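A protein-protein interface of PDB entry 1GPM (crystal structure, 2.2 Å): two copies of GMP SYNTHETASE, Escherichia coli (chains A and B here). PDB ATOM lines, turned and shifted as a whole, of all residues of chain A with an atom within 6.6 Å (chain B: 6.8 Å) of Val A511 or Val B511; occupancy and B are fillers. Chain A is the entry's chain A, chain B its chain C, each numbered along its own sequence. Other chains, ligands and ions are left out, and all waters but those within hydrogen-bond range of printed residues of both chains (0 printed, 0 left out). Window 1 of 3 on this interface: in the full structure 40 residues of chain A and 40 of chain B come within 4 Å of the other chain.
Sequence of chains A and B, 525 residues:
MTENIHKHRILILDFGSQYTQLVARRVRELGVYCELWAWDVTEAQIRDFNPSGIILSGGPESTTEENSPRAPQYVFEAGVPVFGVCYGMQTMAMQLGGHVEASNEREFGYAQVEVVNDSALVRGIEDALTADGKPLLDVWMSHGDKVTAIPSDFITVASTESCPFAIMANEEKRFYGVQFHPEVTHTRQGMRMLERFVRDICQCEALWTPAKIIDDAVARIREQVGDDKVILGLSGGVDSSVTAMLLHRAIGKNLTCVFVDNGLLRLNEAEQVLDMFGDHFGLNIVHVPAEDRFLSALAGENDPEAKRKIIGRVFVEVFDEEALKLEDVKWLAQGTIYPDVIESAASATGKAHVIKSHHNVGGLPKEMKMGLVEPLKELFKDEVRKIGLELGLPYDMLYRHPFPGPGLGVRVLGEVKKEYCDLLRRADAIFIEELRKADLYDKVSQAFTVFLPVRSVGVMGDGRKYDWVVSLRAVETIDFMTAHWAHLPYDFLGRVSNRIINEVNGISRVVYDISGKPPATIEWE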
ATOM      1  N   LEU A 452       1.645 -16.617  28.833  1.00  0.00           N
ATOM      2  CA  LEU A 452       0.729 -15.502  29.093  1.00  0.00           C
ATOM      3  C   LEU A 452       0.331 -15.541  30.556  1.00  0.00           C
ATOM      4  O   LEU A 452      -0.161 -16.557  31.047  1.00  0.00           O
ATOM      5  CB  LEU A 452      -0.548 -15.555  28.224  1.00  0.00           C
ATOM      6  CG  LEU A 452      -0.599 -16.211  26.836  1.00  0.00           C
ATOM      7  CD1 LEU A 452      -1.929 -15.845  26.189  1.00  0.00           C
ATOM      8  CD2 LEU A 452       0.549 -15.801  25.952  1.00  0.00           C
ATOM      9  N   VAL A 469      -1.803 -19.802  30.972  1.00  0.00           N
ATOM     10  CA  VAL A 469      -1.984 -20.051  29.549  1.00  0.00           C
ATOM     11  C   VAL A 469      -0.684 -19.838  28.762  1.00  0.00           C
ATOM     12  O   VAL A 469       0.170 -19.028  29.143  1.00  0.00           O
ATOM     13  CB  VAL A 469      -3.049 -19.078  28.982  1.00  0.00           C
ATOM     14  CG1 VAL A 469      -3.370 -19.393  27.520  1.00  0.00           C
ATOM     15  CG2 VAL A 469      -4.301 -19.110  29.837  1.00  0.00           C
ATOM     16  N   VAL A 470      -0.517 -20.603  27.690  1.00  0.00           N
ATOM     17  CA  VAL A 470       0.641 -20.439  26.821  1.00  0.00           C
ATOM     18  C   VAL A 470       0.140 -20.388  25.392  1.00  0.00           C
ATOM     19  O   VAL A 470      -0.950 -20.892  25.086  1.00  0.00           O
ATOM     20  CB  VAL A 470       1.695 -21.562  26.947  1.00  0.00           C
ATOM     21  CG1 VAL A 470       2.292 -21.574  28.341  1.00  0.00           C
ATOM     22  CG2 VAL A 470       1.111 -22.910  26.567  1.00  0.00           C
ATOM     23  N   SER A 471       0.886 -19.703  24.536  1.00  0.00           N
ATOM     24  CA  SER A 471       0.521 -19.613  23.131  1.00  0.00           C
ATOM     25  C   SER A 471       1.608 -20.239  22.298  1.00  0.00           C
ATOM     26  O   SER A 471       2.796 -20.062  22.574  1.00  0.00           O
ATOM     27  CB  SER A 471       0.333 -18.166  22.686  1.00  0.00           C
ATOM     28  OG  SER A 471      -0.119 -18.116  21.341  1.00  0.00           O
ATOM     29  N   LEU A 472       1.190 -21.074  21.358  1.00  0.00           N
ATOM     30  CA  LEU A 472       2.111 -21.709  20.435  1.00  0.00           C
ATOM     31  C   LEU A 472       2.303 -20.693  19.314  1.00  0.00           C
ATOM     32  O   LEU A 472       1.377 -19.947  18.971  1.00  0.00           O
ATOM     33  CB  LEU A 472       1.505 -22.976  19.865  1.00  0.00           C
ATOM     34  CG  LEU A 472       1.189 -24.059  20.878  1.00  0.00           C
ATOM     35  CD1 LEU A 472       0.730 -25.311  20.133  1.00  0.00           C
ATOM     36  CD2 LEU A 472       2.424 -24.339  21.737  1.00  0.00           C
ATOM     37  N   ARG A 473       3.497 -20.654  18.744  1.00  0.00           N
ATOM     38  CA  ARG A 473       3.786 -19.701  17.677  1.00  0.00           C
ATOM     39  C   ARG A 473       4.659 -20.387  16.645  1.00  0.00           C
ATOM     40  O   ARG A 473       5.651 -21.022  16.991  1.00  0.00           O
ATOM     41  CB  ARG A 473       4.476 -18.460  18.287  1.00  0.00           C
ATOM     42  CG  ARG A 473       4.913 -17.352  17.339  1.00  0.00           C
ATOM     43  CD  ARG A 473       3.861 -17.005  16.358  1.00  0.00           C
ATOM     44  NE  ARG A 473       4.002 -15.654  15.833  1.00  0.00           N
ATOM     45  CZ  ARG A 473       3.271 -15.187  14.829  1.00  0.00           C
ATOM     46  NH1 ARG A 473       2.390 -15.988  14.256  1.00  0.00           N
ATOM     47  NH2 ARG A 473       3.334 -13.904  14.479  1.00  0.00           N
ATOM     48  N   SER A 497      -1.660 -29.607  22.385  1.00  0.00           N
ATOM     49  CA  SER A 497      -2.536 -28.950  23.332  1.00  0.00           C
ATOM     50  C   SER A 497      -2.835 -29.908  24.477  1.00  0.00           C
ATOM     51  O   SER A 497      -2.644 -29.575  25.651  1.00  0.00           O
ATOM     52  CB  SER A 497      -3.837 -28.568  22.638  1.00  0.00           C
ATOM     53  OG  SER A 497      -4.726 -27.964  23.553  1.00  0.00           O
ATOM     54  N   ARG A 509      -4.587 -24.134  29.746  1.00  0.00           N
ATOM     55  CA  ARG A 509      -5.068 -23.779  28.416  1.00  0.00           C
ATOM     56  C   ARG A 509      -3.940 -23.468  27.449  1.00  0.00           C
ATOM     57  O   ARG A 509      -2.926 -22.878  27.828  1.00  0.00           O
ATOM     58  CB  ARG A 509      -6.007 -22.578  28.492  1.00  0.00           C
ATOM     59  CG  ARG A 509      -6.797 -22.365  27.214  1.00  0.00           C
ATOM     60  CD  ARG A 509      -7.971 -21.466  27.446  1.00  0.00           C
ATOM     61  NE  ARG A 509      -8.807 -21.941  28.546  1.00  0.00           N
ATOM     62  CZ  ARG A 509     -10.055 -22.376  28.414  1.00  0.00           C
ATOM     63  NH1 ARG A 509     -10.631 -22.412  27.221  1.00  0.00           N
ATOM     64  NH2 ARG A 509     -10.744 -22.721  29.494  1.00  0.00           N
ATOM     65  N   VAL A 510      -4.125 -23.870  26.197  1.00  0.00           N
ATOM     66  CA  VAL A 510      -3.142 -23.626  25.158  1.00  0.00           C
ATOM     67  C   VAL A 510      -3.867 -22.963  24.002  1.00  0.00           C
ATOM     68  O   VAL A 510      -4.981 -23.371  23.656  1.00  0.00           O
ATOM     69  CB  VAL A 510      -2.461 -24.937  24.687  1.00  0.00           C
ATOM     70  CG1 VAL A 510      -1.498 -24.663  23.537  1.00  0.00           C
ATOM     71  CG2 VAL A 510      -1.716 -25.579  25.850  1.00  0.00           C
ATOM     72  N   VAL A 511      -3.256 -21.915  23.449  1.00  0.00           N
ATOM     73  CA  VAL A 511      -3.825 -21.178  22.316  1.00  0.00           C
ATOM     74  C   VAL A 511      -2.808 -21.145  21.176  1.00  0.00           C
ATOM     75  O   VAL A 511      -1.627 -21.423  21.381  1.00  0.00           O
ATOM     76  CB  VAL A 511      -4.194 -19.711  22.687  1.00  0.00           C
ATOM     77  CG1 VAL A 511      -5.299 -19.681  23.735  1.00  0.00           C
ATOM     78  CG2 VAL A 511      -2.971 -18.975  23.174  1.00  0.00           C
ATOM     79  N   TYR A 512      -3.263 -20.792  19.982  1.00  0.00           N
ATOM     80  CA  TYR A 512      -2.372 -20.743  18.837  1.00  0.00           C
ATOM     81  C   TYR A 512      -2.385 -19.364  18.190  1.00  0.00           C
ATOM     82  O   TYR A 512      -3.453 -18.798  17.969  1.00  0.00           O
ATOM     83  CB  TYR A 512      -2.770 -21.808  17.819  1.00  0.00           C
ATOM     84  CG  TYR A 512      -1.800 -21.891  16.670  1.00  0.00           C
ATOM     85  CD1 TYR A 512      -0.457 -22.191  16.897  1.00  0.00           C
ATOM     86  CD2 TYR A 512      -2.211 -21.658  15.366  1.00  0.00           C
ATOM     87  CE1 TYR A 512       0.447 -22.252  15.857  1.00  0.00           C
ATOM     88  CE2 TYR A 512      -1.311 -21.721  14.313  1.00  0.00           C
ATOM     89  CZ  TYR A 512       0.016 -22.018  14.566  1.00  0.00           C
ATOM     90  OH  TYR A 512       0.921 -22.098  13.536  1.00  0.00           O
ATOM     91  N   ASP A 513      -1.199 -18.821  17.903  1.00  0.00           N
ATOM     92  CA  ASP A 513      -1.092 -17.504  17.284  1.00  0.00           C
ATOM     93  C   ASP A 513      -1.449 -17.569  15.803  1.00  0.00           C
ATOM     94  O   ASP A 513      -0.803 -18.280  15.024  1.00  0.00           O
ATOM     95  CB  ASP A 513       0.310 -16.913  17.464  1.00  0.00           C
ATOM     96  CG  ASP A 513       0.365 -15.420  17.142  1.00  0.00           C
ATOM     97  OD1 ASP A 513      -0.638 -14.860  16.647  1.00  0.00           O
ATOM     98  OD2 ASP A 513       1.412 -14.789  17.393  1.00  0.00           O
ATOM     99  N   ILE A 514      -2.489 -16.836  15.421  1.00  0.00           N
ATOM    100  CA  ILE A 514      -2.934 -16.828  14.039  1.00  0.00           C
ATOM    101  C   ILE A 514      -2.778 -15.443  13.444  1.00  0.00           C
ATOM    102  O   ILE A 514      -3.532 -15.043  12.558  1.00  0.00           O
ATOM    103  CB  ILE A 514      -4.406 -17.333  13.885  1.00  0.00           C
ATOM    104  CG1 ILE A 514      -5.372 -16.496  14.747  1.00  0.00           C
ATOM    105  CG2 ILE A 514      -4.466 -18.824  14.219  1.00  0.00           C
ATOM    106  CD1 ILE A 514      -6.853 -16.661  14.419  1.00  0.00           C
ATOM    107  N   SER A 515      -1.787 -14.714  13.941  1.00  0.00           N
ATOM    108  CA  SER A 515      -1.498 -13.372  13.460  1.00  0.00           C
ATOM    109  C   SER A 515      -0.246 -13.462  12.599  1.00  0.00           C
ATOM    110  O   SER A 515       0.770 -14.016  13.025  1.00  0.00           O
ATOM    111  CB  SER A 515      -1.245 -12.441  14.640  1.00  0.00           C
ATOM    112  OG  SER A 515      -2.336 -12.452  15.541  1.00  0.00           O
ATOM    113  N   TRP A 524       6.422 -11.655  20.344  1.00  0.00           N
ATOM    114  CA  TRP A 524       5.399 -10.845  20.988  1.00  0.00           C
ATOM    115  C   TRP A 524       5.950  -9.624  21.710  1.00  0.00           C
ATOM    116  O   TRP A 524       5.184  -8.709  22.038  1.00  0.00           O
ATOM    117  CB  TRP A 524       4.619 -11.676  21.995  1.00  0.00           C
ATOM    118  CG  TRP A 524       3.689 -12.670  21.401  1.00  0.00           C
ATOM    119  CD1 TRP A 524       3.926 -13.504  20.335  1.00  0.00           C
ATOM    120  CD2 TRP A 524       2.384 -12.993  21.887  1.00  0.00           C
ATOM    121  NE1 TRP A 524       2.846 -14.330  20.138  1.00  0.00           N
ATOM    122  CE2 TRP A 524       1.889 -14.043  21.074  1.00  0.00           C
ATOM    123  CE3 TRP A 524       1.590 -12.504  22.933  1.00  0.00           C
ATOM    124  CZ2 TRP A 524       0.622 -14.614  21.286  1.00  0.00           C
ATOM    125  CZ3 TRP A 524       0.337 -13.067  23.144  1.00  0.00           C
ATOM    126  CH2 TRP A 524      -0.135 -14.116  22.321  1.00  0.00           C
ATOM    127  N   LEU B 452      -7.672 -10.617  26.449  1.00  0.00           N
ATOM    128  CA  LEU B 452      -6.528 -10.953  27.273  1.00  0.00           C
ATOM    129  C   LEU B 452      -5.795  -9.685  27.712  1.00  0.00           C
ATOM    130  O   LEU B 452      -5.419  -8.847  26.884  1.00  0.00           O
ATOM    131  CB  LEU B 452      -5.574 -11.894  26.528  1.00  0.00           C
ATOM    132  CG  LEU B 452      -6.177 -13.088  25.779  1.00  0.00           C
ATOM    133  CD1 LEU B 452      -5.076 -14.028  25.368  1.00  0.00           C
ATOM    134  CD2 LEU B 452      -7.156 -13.832  26.651  1.00  0.00           C
ATOM    135  N   VAL B 469      -4.312  -8.044  23.297  1.00  0.00           N
ATOM    136  CA  VAL B 469      -4.493  -9.317  22.591  1.00  0.00           C
ATOM    137  C   VAL B 469      -5.884  -9.863  22.878  1.00  0.00           C
ATOM    138  O   VAL B 469      -6.443  -9.618  23.958  1.00  0.00           O
ATOM    139  CB  VAL B 469      -3.486 -10.406  23.092  1.00  0.00           C
ATOM    140  CG1 VAL B 469      -3.513 -11.614  22.187  1.00  0.00           C
ATOM    141  CG2 VAL B 469      -2.079  -9.851  23.165  1.00  0.00           C
ATOM    142  N   VAL B 470      -6.448 -10.575  21.904  1.00  0.00           N
ATOM    143  CA  VAL B 470      -7.755 -11.210  22.059  1.00  0.00           C
ATOM    144  C   VAL B 470      -7.644 -12.677  21.614  1.00  0.00           C
ATOM    145  O   VAL B 470      -6.727 -13.051  20.885  1.00  0.00           O
ATOM    146  CB  VAL B 470      -8.893 -10.462  21.290  1.00  0.00           C
ATOM    147  CG1 VAL B 470      -9.060  -9.045  21.837  1.00  0.00           C
ATOM    148  CG2 VAL B 470      -8.615 -10.429  19.796  1.00  0.00           C
ATOM    149  N   SER B 471      -8.532 -13.520  22.119  1.00  0.00           N
ATOM    150  CA  SER B 471      -8.528 -14.929  21.784  1.00  0.00           C
ATOM    151  C   SER B 471      -9.884 -15.313  21.217  1.00  0.00           C
ATOM    152  O   SER B 471     -10.925 -14.877  21.731  1.00  0.00           O
ATOM    153  CB  SER B 471      -8.235 -15.758  23.033  1.00  0.00           C
ATOM    154  OG  SER B 471      -8.000 -17.109  22.699  1.00  0.00           O
ATOM    155  N   LEU B 472      -9.871 -16.079  20.129  1.00  0.00           N
ATOM    156  CA  LEU B 472     -11.108 -16.538  19.515  1.00  0.00           C
ATOM    157  C   LEU B 472     -11.410 -17.926  20.088  1.00  0.00           C
ATOM    158  O   LEU B 472     -10.522 -18.784  20.178  1.00  0.00           O
ATOM    159  CB  LEU B 472     -10.981 -16.603  17.988  1.00  0.00           C
ATOM    160  CG  LEU B 472     -10.625 -15.307  17.255  1.00  0.00           C
ATOM    161  CD1 LEU B 472     -10.762 -15.506  15.758  1.00  0.00           C
ATOM    162  CD2 LEU B 472     -11.524 -14.186  17.711  1.00  0.00           C
ATOM    163  N   ARG B 473     -12.655 -18.133  20.489  1.00  0.00           N
ATOM    164  CA  ARG B 473     -13.077 -19.397  21.081  1.00  0.00           C
ATOM    165  C   ARG B 473     -14.311 -19.930  20.355  1.00  0.00           C
ATOM    166  O   ARG B 473     -15.359 -19.274  20.322  1.00  0.00           O
ATOM    167  CB  ARG B 473     -13.360 -19.183  22.573  1.00  0.00           C
ATOM    168  CG  ARG B 473     -13.823 -20.407  23.351  1.00  0.00           C
ATOM    169  CD  ARG B 473     -12.906 -21.561  23.122  1.00  0.00           C
ATOM    170  NE  ARG B 473     -12.909 -22.531  24.203  1.00  0.00           N
ATOM    171  CZ  ARG B 473     -12.355 -23.734  24.094  1.00  0.00           C
ATOM    172  NH1 ARG B 473     -11.786 -24.083  22.943  1.00  0.00           N
ATOM    173  NH2 ARG B 473     -12.314 -24.560  25.140  1.00  0.00           N
ATOM    174  N   SER B 497      -8.436 -12.640  11.837  1.00  0.00           N
ATOM    175  CA  SER B 497      -7.374 -11.982  12.593  1.00  0.00           C
ATOM    176  C   SER B 497      -6.894 -10.750  11.860  1.00  0.00           C
ATOM    177  O   SER B 497      -6.588  -9.723  12.478  1.00  0.00           O
ATOM    178  CB  SER B 497      -6.211 -12.935  12.899  1.00  0.00           C
ATOM    179  OG  SER B 497      -5.690 -13.533  11.729  1.00  0.00           O
ATOM    180  N   ARG B 509      -2.699  -8.267  18.332  1.00  0.00           N
ATOM    181  CA  ARG B 509      -2.607  -9.680  18.009  1.00  0.00           C
ATOM    182  C   ARG B 509      -3.850 -10.479  18.354  1.00  0.00           C
ATOM    183  O   ARG B 509      -4.542 -10.199  19.336  1.00  0.00           O
ATOM    184  CB  ARG B 509      -1.399 -10.277  18.735  1.00  0.00           C
ATOM    185  CG  ARG B 509      -0.956 -11.616  18.227  1.00  0.00           C
ATOM    186  CD  ARG B 509       0.341 -12.035  18.861  1.00  0.00           C
ATOM    187  NE  ARG B 509       1.412 -11.050  18.682  1.00  0.00           N
ATOM    188  CZ  ARG B 509       2.539 -11.278  18.014  1.00  0.00           C
ATOM    189  NH1 ARG B 509       2.736 -12.459  17.433  1.00  0.00           N
ATOM    190  NH2 ARG B 509       3.511 -10.361  18.024  1.00  0.00           N
ATOM    191  N   VAL B 510      -4.052 -11.545  17.586  1.00  0.00           N
ATOM    192  CA  VAL B 510      -5.188 -12.443  17.737  1.00  0.00           C
ATOM    193  C   VAL B 510      -4.718 -13.898  17.794  1.00  0.00           C
ATOM    194  O   VAL B 510      -3.898 -14.337  16.975  1.00  0.00           O
ATOM    195  CB  VAL B 510      -6.176 -12.242  16.557  1.00  0.00           C
ATOM    196  CG1 VAL B 510      -7.357 -13.175  16.674  1.00  0.00           C
ATOM    197  CG2 VAL B 510      -6.653 -10.800  16.548  1.00  0.00           C
ATOM    198  N   VAL B 511      -5.178 -14.616  18.817  1.00  0.00           N
ATOM    199  CA  VAL B 511      -4.838 -16.029  18.988  1.00  0.00           C
ATOM    200  C   VAL B 511      -6.137 -16.836  18.900  1.00  0.00           C
ATOM    201  O   VAL B 511      -7.219 -16.266  18.935  1.00  0.00           O
ATOM    202  CB  VAL B 511      -4.109 -16.301  20.348  1.00  0.00           C
ATOM    203  CG1 VAL B 511      -2.890 -15.395  20.481  1.00  0.00           C
ATOM    204  CG2 VAL B 511      -5.043 -16.105  21.533  1.00  0.00           C
ATOM    205  N   TYR B 512      -6.031 -18.147  18.740  1.00  0.00           N
ATOM    206  CA  TYR B 512      -7.208 -19.004  18.655  1.00  0.00           C
ATOM    207  C   TYR B 512      -7.069 -20.152  19.659  1.00  0.00           C
ATOM    208  O   TYR B 512      -6.068 -20.871  19.650  1.00  0.00           O
ATOM    209  CB  TYR B 512      -7.360 -19.555  17.235  1.00  0.00           C
ATOM    210  CG  TYR B 512      -8.527 -20.500  17.093  1.00  0.00           C
ATOM    211  CD1 TYR B 512      -9.832 -20.043  17.234  1.00  0.00           C
ATOM    212  CD2 TYR B 512      -8.325 -21.866  16.904  1.00  0.00           C
ATOM    213  CE1 TYR B 512     -10.902 -20.919  17.204  1.00  0.00           C
ATOM    214  CE2 TYR B 512      -9.389 -22.752  16.872  1.00  0.00           C
ATOM    215  CZ  TYR B 512     -10.671 -22.273  17.027  1.00  0.00           C
ATOM    216  OH  TYR B 512     -11.727 -23.143  17.051  1.00  0.00           O
ATOM    217  N   ASP B 513      -8.066 -20.308  20.523  1.00  0.00           N
ATOM    218  CA  ASP B 513      -8.074 -21.353  21.556  1.00  0.00           C
ATOM    219  C   ASP B 513      -8.136 -22.779  20.967  1.00  0.00           C
ATOM    220  O   ASP B 513      -9.097 -23.140  20.270  1.00  0.00           O
ATOM    221  CB  ASP B 513      -9.272 -21.102  22.492  1.00  0.00           C
ATOM    222  CG  ASP B 513      -9.200 -21.881  23.803  1.00  0.00           C
ATOM    223  OD1 ASP B 513      -8.499 -22.910  23.905  1.00  0.00           O
ATOM    224  OD2 ASP B 513      -9.900 -21.470  24.750  1.00  0.00           O
ATOM    225  N   ILE B 514      -7.096 -23.573  21.216  1.00  0.00           N
ATOM    226  CA  ILE B 514      -7.064 -24.950  20.731  1.00  0.00           C
ATOM    227  C   ILE B 514      -7.129 -25.928  21.899  1.00  0.00           C
ATOM    228  O   ILE B 514      -6.487 -26.965  21.886  1.00  0.00           O
ATOM    229  CB  ILE B 514      -5.800 -25.277  19.858  1.00  0.00           C
ATOM    230  CG1 ILE B 514      -4.518 -25.049  20.660  1.00  0.00           C
ATOM    231  CG2 ILE B 514      -5.801 -24.437  18.584  1.00  0.00           C
ATOM    232  CD1 ILE B 514      -3.276 -25.522  19.967  1.00  0.00           C
ATOM    233  N   SER B 515      -7.902 -25.592  22.918  1.00  0.00           N
ATOM    234  CA  SER B 515      -8.042 -26.467  24.069  1.00  0.00           C
ATOM    235  C   SER B 515      -9.421 -27.131  24.030  1.00  0.00           C
ATOM    236  O   SER B 515     -10.459 -26.455  23.857  1.00  0.00           O
ATOM    237  CB  SER B 515      -7.872 -25.669  25.362  1.00  0.00           C
ATOM    238  OG  SER B 515      -6.622 -25.006  25.404  1.00  0.00           O
ATOM    239  N   TRP B 524     -13.260 -19.275  29.660  1.00  0.00           N
ATOM    240  CA  TRP B 524     -11.967 -19.154  30.316  1.00  0.00           C
ATOM    241  C   TRP B 524     -12.051 -18.996  31.823  1.00  0.00           C
ATOM    242  O   TRP B 524     -11.269 -19.620  32.552  1.00  0.00           O
ATOM    243  CB  TRP B 524     -11.169 -18.002  29.710  1.00  0.00           C
ATOM    244  CG  TRP B 524     -10.569 -18.341  28.382  1.00  0.00           C
ATOM    245  CD1 TRP B 524     -11.150 -19.057  27.366  1.00  0.00           C
ATOM    246  CD2 TRP B 524      -9.263 -17.989  27.929  1.00  0.00           C
ATOM    247  NE1 TRP B 524     -10.278 -19.169  26.310  1.00  0.00           N
ATOM    248  CE2 TRP B 524      -9.111 -18.521  26.627  1.00  0.00           C
ATOM    249  CE3 TRP B 524      -8.194 -17.275  28.492  1.00  0.00           C
ATOM    250  CZ2 TRP B 524      -7.941 -18.359  25.884  1.00  0.00           C
ATOM    251  CZ3 TRP B 524      -7.032 -17.116  27.752  1.00  0.00           C
ATOM    252  CH2 TRP B 524      -6.917 -17.656  26.462  1.00  0.00           C
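O of Ile A514 lies within hydrogen-bond range of OG of Ser B497, at 2.8 Å. O of Tyr A512 sits at hydrogen-bond distance from N of Tyr B512 (2.8 Å). The guanidinium group (NH1) of Arg B509 lies close to the indole nitrogen (NE1) of Trp A524, at 3.3 Å. The backbone NH (N) of Val A510 lies within hydrogen-bond range of the side-chain hydroxyl (OG) of Ser B515 (2.9 Å). NE1 of Trp B524 lies close to NH1 of Arg A509, 3.4 Å away. The guanidinium group (NH1) of Arg A509 sits close to the guanidinium group (NH2) of Arg B473 (3.4 Å). O of Val B510 sits close to OD1 of Asp A513 (3.3 Å). The guanidinium group (NH2) of Arg A473 lies close to the guanidinium group (NH1) of Arg B509 (3.3 Å). N of Ile A514 sits at hydrogen-bond distance from O of Val B510. NH1 of Arg A509 is in salt-bridge range of OD2 of Asp B513, at 2.7 Å. The side-chain hydroxyl (OG) of Ser A497 is in hydrogen-bond range of the backbone carbonyl oxygen (O) of Ile B514 (2.6 Å). The side-chain carboxylate of Asp A513 is in salt-bridge range of the guanidinium group of Arg B509 (2.7 Å). N of Ile B514 sits at hydrogen-bond distance from O of Val A510. The side-chain hydroxyl (OG) of Ser A515 sits at hydrogen-bond distance from the backbone NH (N) of Val B510, at 2.8 Å.
The guanidinium group (NH1) of Arg B473 lies within hydrogen-bond range of the backbone carbonyl oxygen (O) of Ser B515 (2.9 Å). N of Asp B513 sits at hydrogen-bond distance from O of Leu B472, 2.9 Å away. The side-chain carboxylate of Asp A513 is in hydrogen-bond range of the indole nitrogen of Trp A524. The backbone NH (N) of Asp A513 is in hydrogen-bond range of the backbone carbonyl oxygen (O) of Leu A472. The side-chain carboxylate (OD1) of Asp A513 lies within hydrogen-bond range of the backbone NH (N) of Ser A515. NE of Arg A473 lies within salt-bridge range of OD2 of Asp A513 (3.1 Å).
Leu A452 touches Leu B452 (CD1 to CD1, 3.7 Å). Val B511 touches Ser A471 (CG1 to OG, 3.98 Å). Ser B515 touches Ser A497 (CA to OG, 3.7 Å). OG of Ser B515 touches CG of Arg A509 (3.2 Å). O of Val A510 touches OD1 of Asp B513 (3.6 Å). Val B511 touches Val A511 (CG2 to CB, 3.9 Å). Val A511 touches Tyr B512 (CA to O, 3.5 Å). CG1 of Val A511 touches CA of Asp B513, 3.9 Å away. OG of Ser A515 touches CG of Arg B509 (3.1 Å). Trp A524 touches Val B511.
Val A511 touches just these residues of chain B: Ser B471 (3.9 Å), Val B511 (3.9 Å), Tyr B512 (3.5 Å), Asp B513 (3.9 Å) and Trp B524 (3.7 Å). Val B511 touches just these residues of chain A: Ser A471 (3.98 Å), Val A511 (3.9 Å), Tyr A512 (3.3 Å) and Trp A524 (3.6 Å). Of the printed residues of chain B, Trp A524 touches Arg B509 (3.3 Å) and Val B511 (3.6 Å). Printed residues of chain A within 4 Å of Ser B515: Ser A497, Arg A509 and Val A510. Of the printed residues of chain B, Ser A515 touches Arg B509 (3.1 Å) and Val B510 (2.8 Å). Printed residues of chain B within 4 Å of Arg A473: Arg B509. Printed residues of chain A within 4 Å of Val B510: Asp A513, Ile A514 and Ser A515. Val B470 touches none of the printed residues of chain A. Val A470 touches none of the printed residues of chain B. The nearest residue of chain B that does not touch Val A511 is Ile B514 (4.2 Å). The nearest printed residue of chain B that does not touch Leu A452 is Trp B524 (5.3 Å).
Printed residues of chain A that touch a printed residue of chain B: Leu A452, Val A469, Ser A471, Arg A473, Ser A497, Arg A509, Val A510, Val A511, Tyr A512, Asp A513, Ile A514, Ser A515 and Trp A524. Hydrophobic or aromatic side chains of chain A within 4 Å of the printed part of chain B: Leu A452, Val A469, Val A511, Tyr A512, Ile A514 and Trp A524. Printed residues of chain B that touch a printed residue of chain A: Leu B452, Ser B471, Arg B473, Ser B497, Arg B509, Val B510, Val B511, Tyr B512, Asp B513, Ile B514, Ser B515 and Trp B524. Hydrophobic or aromatic side chains of chain B that line the printed part of chain A: Leu B452, Val B510, Val B511, Ile B514 and Trp B524. Among the printed residues, 28 pairs touch across the chains. Among the printed residues, Asp or Glu carboxylates within 4 Å of a Lys or Arg side-chain nitrogen of the other chain: Arg A509 with Asp B513 (2.7 Å) and Asp A513 with Arg B509 (2.7 Å).
Ser A497 touches Ile B514, and with the chains exchanged Ile A514 touches Ser B497. Val A510 touches Ile B514, and with the chains exchanged Ile A514 touches Val B510. Val A511 touches Asp B513, but with the chains exchanged Asp A513 does not touch Val B511 (4.2 Å). Val A511 touches Trp B524, and with the chains exchanged Trp A524 touches Val B511. 15 positions are printed for both chains. Of the 28 pairs that touch across the chains among the printed residues, 25 have their exchanged pair printed and touching as well.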
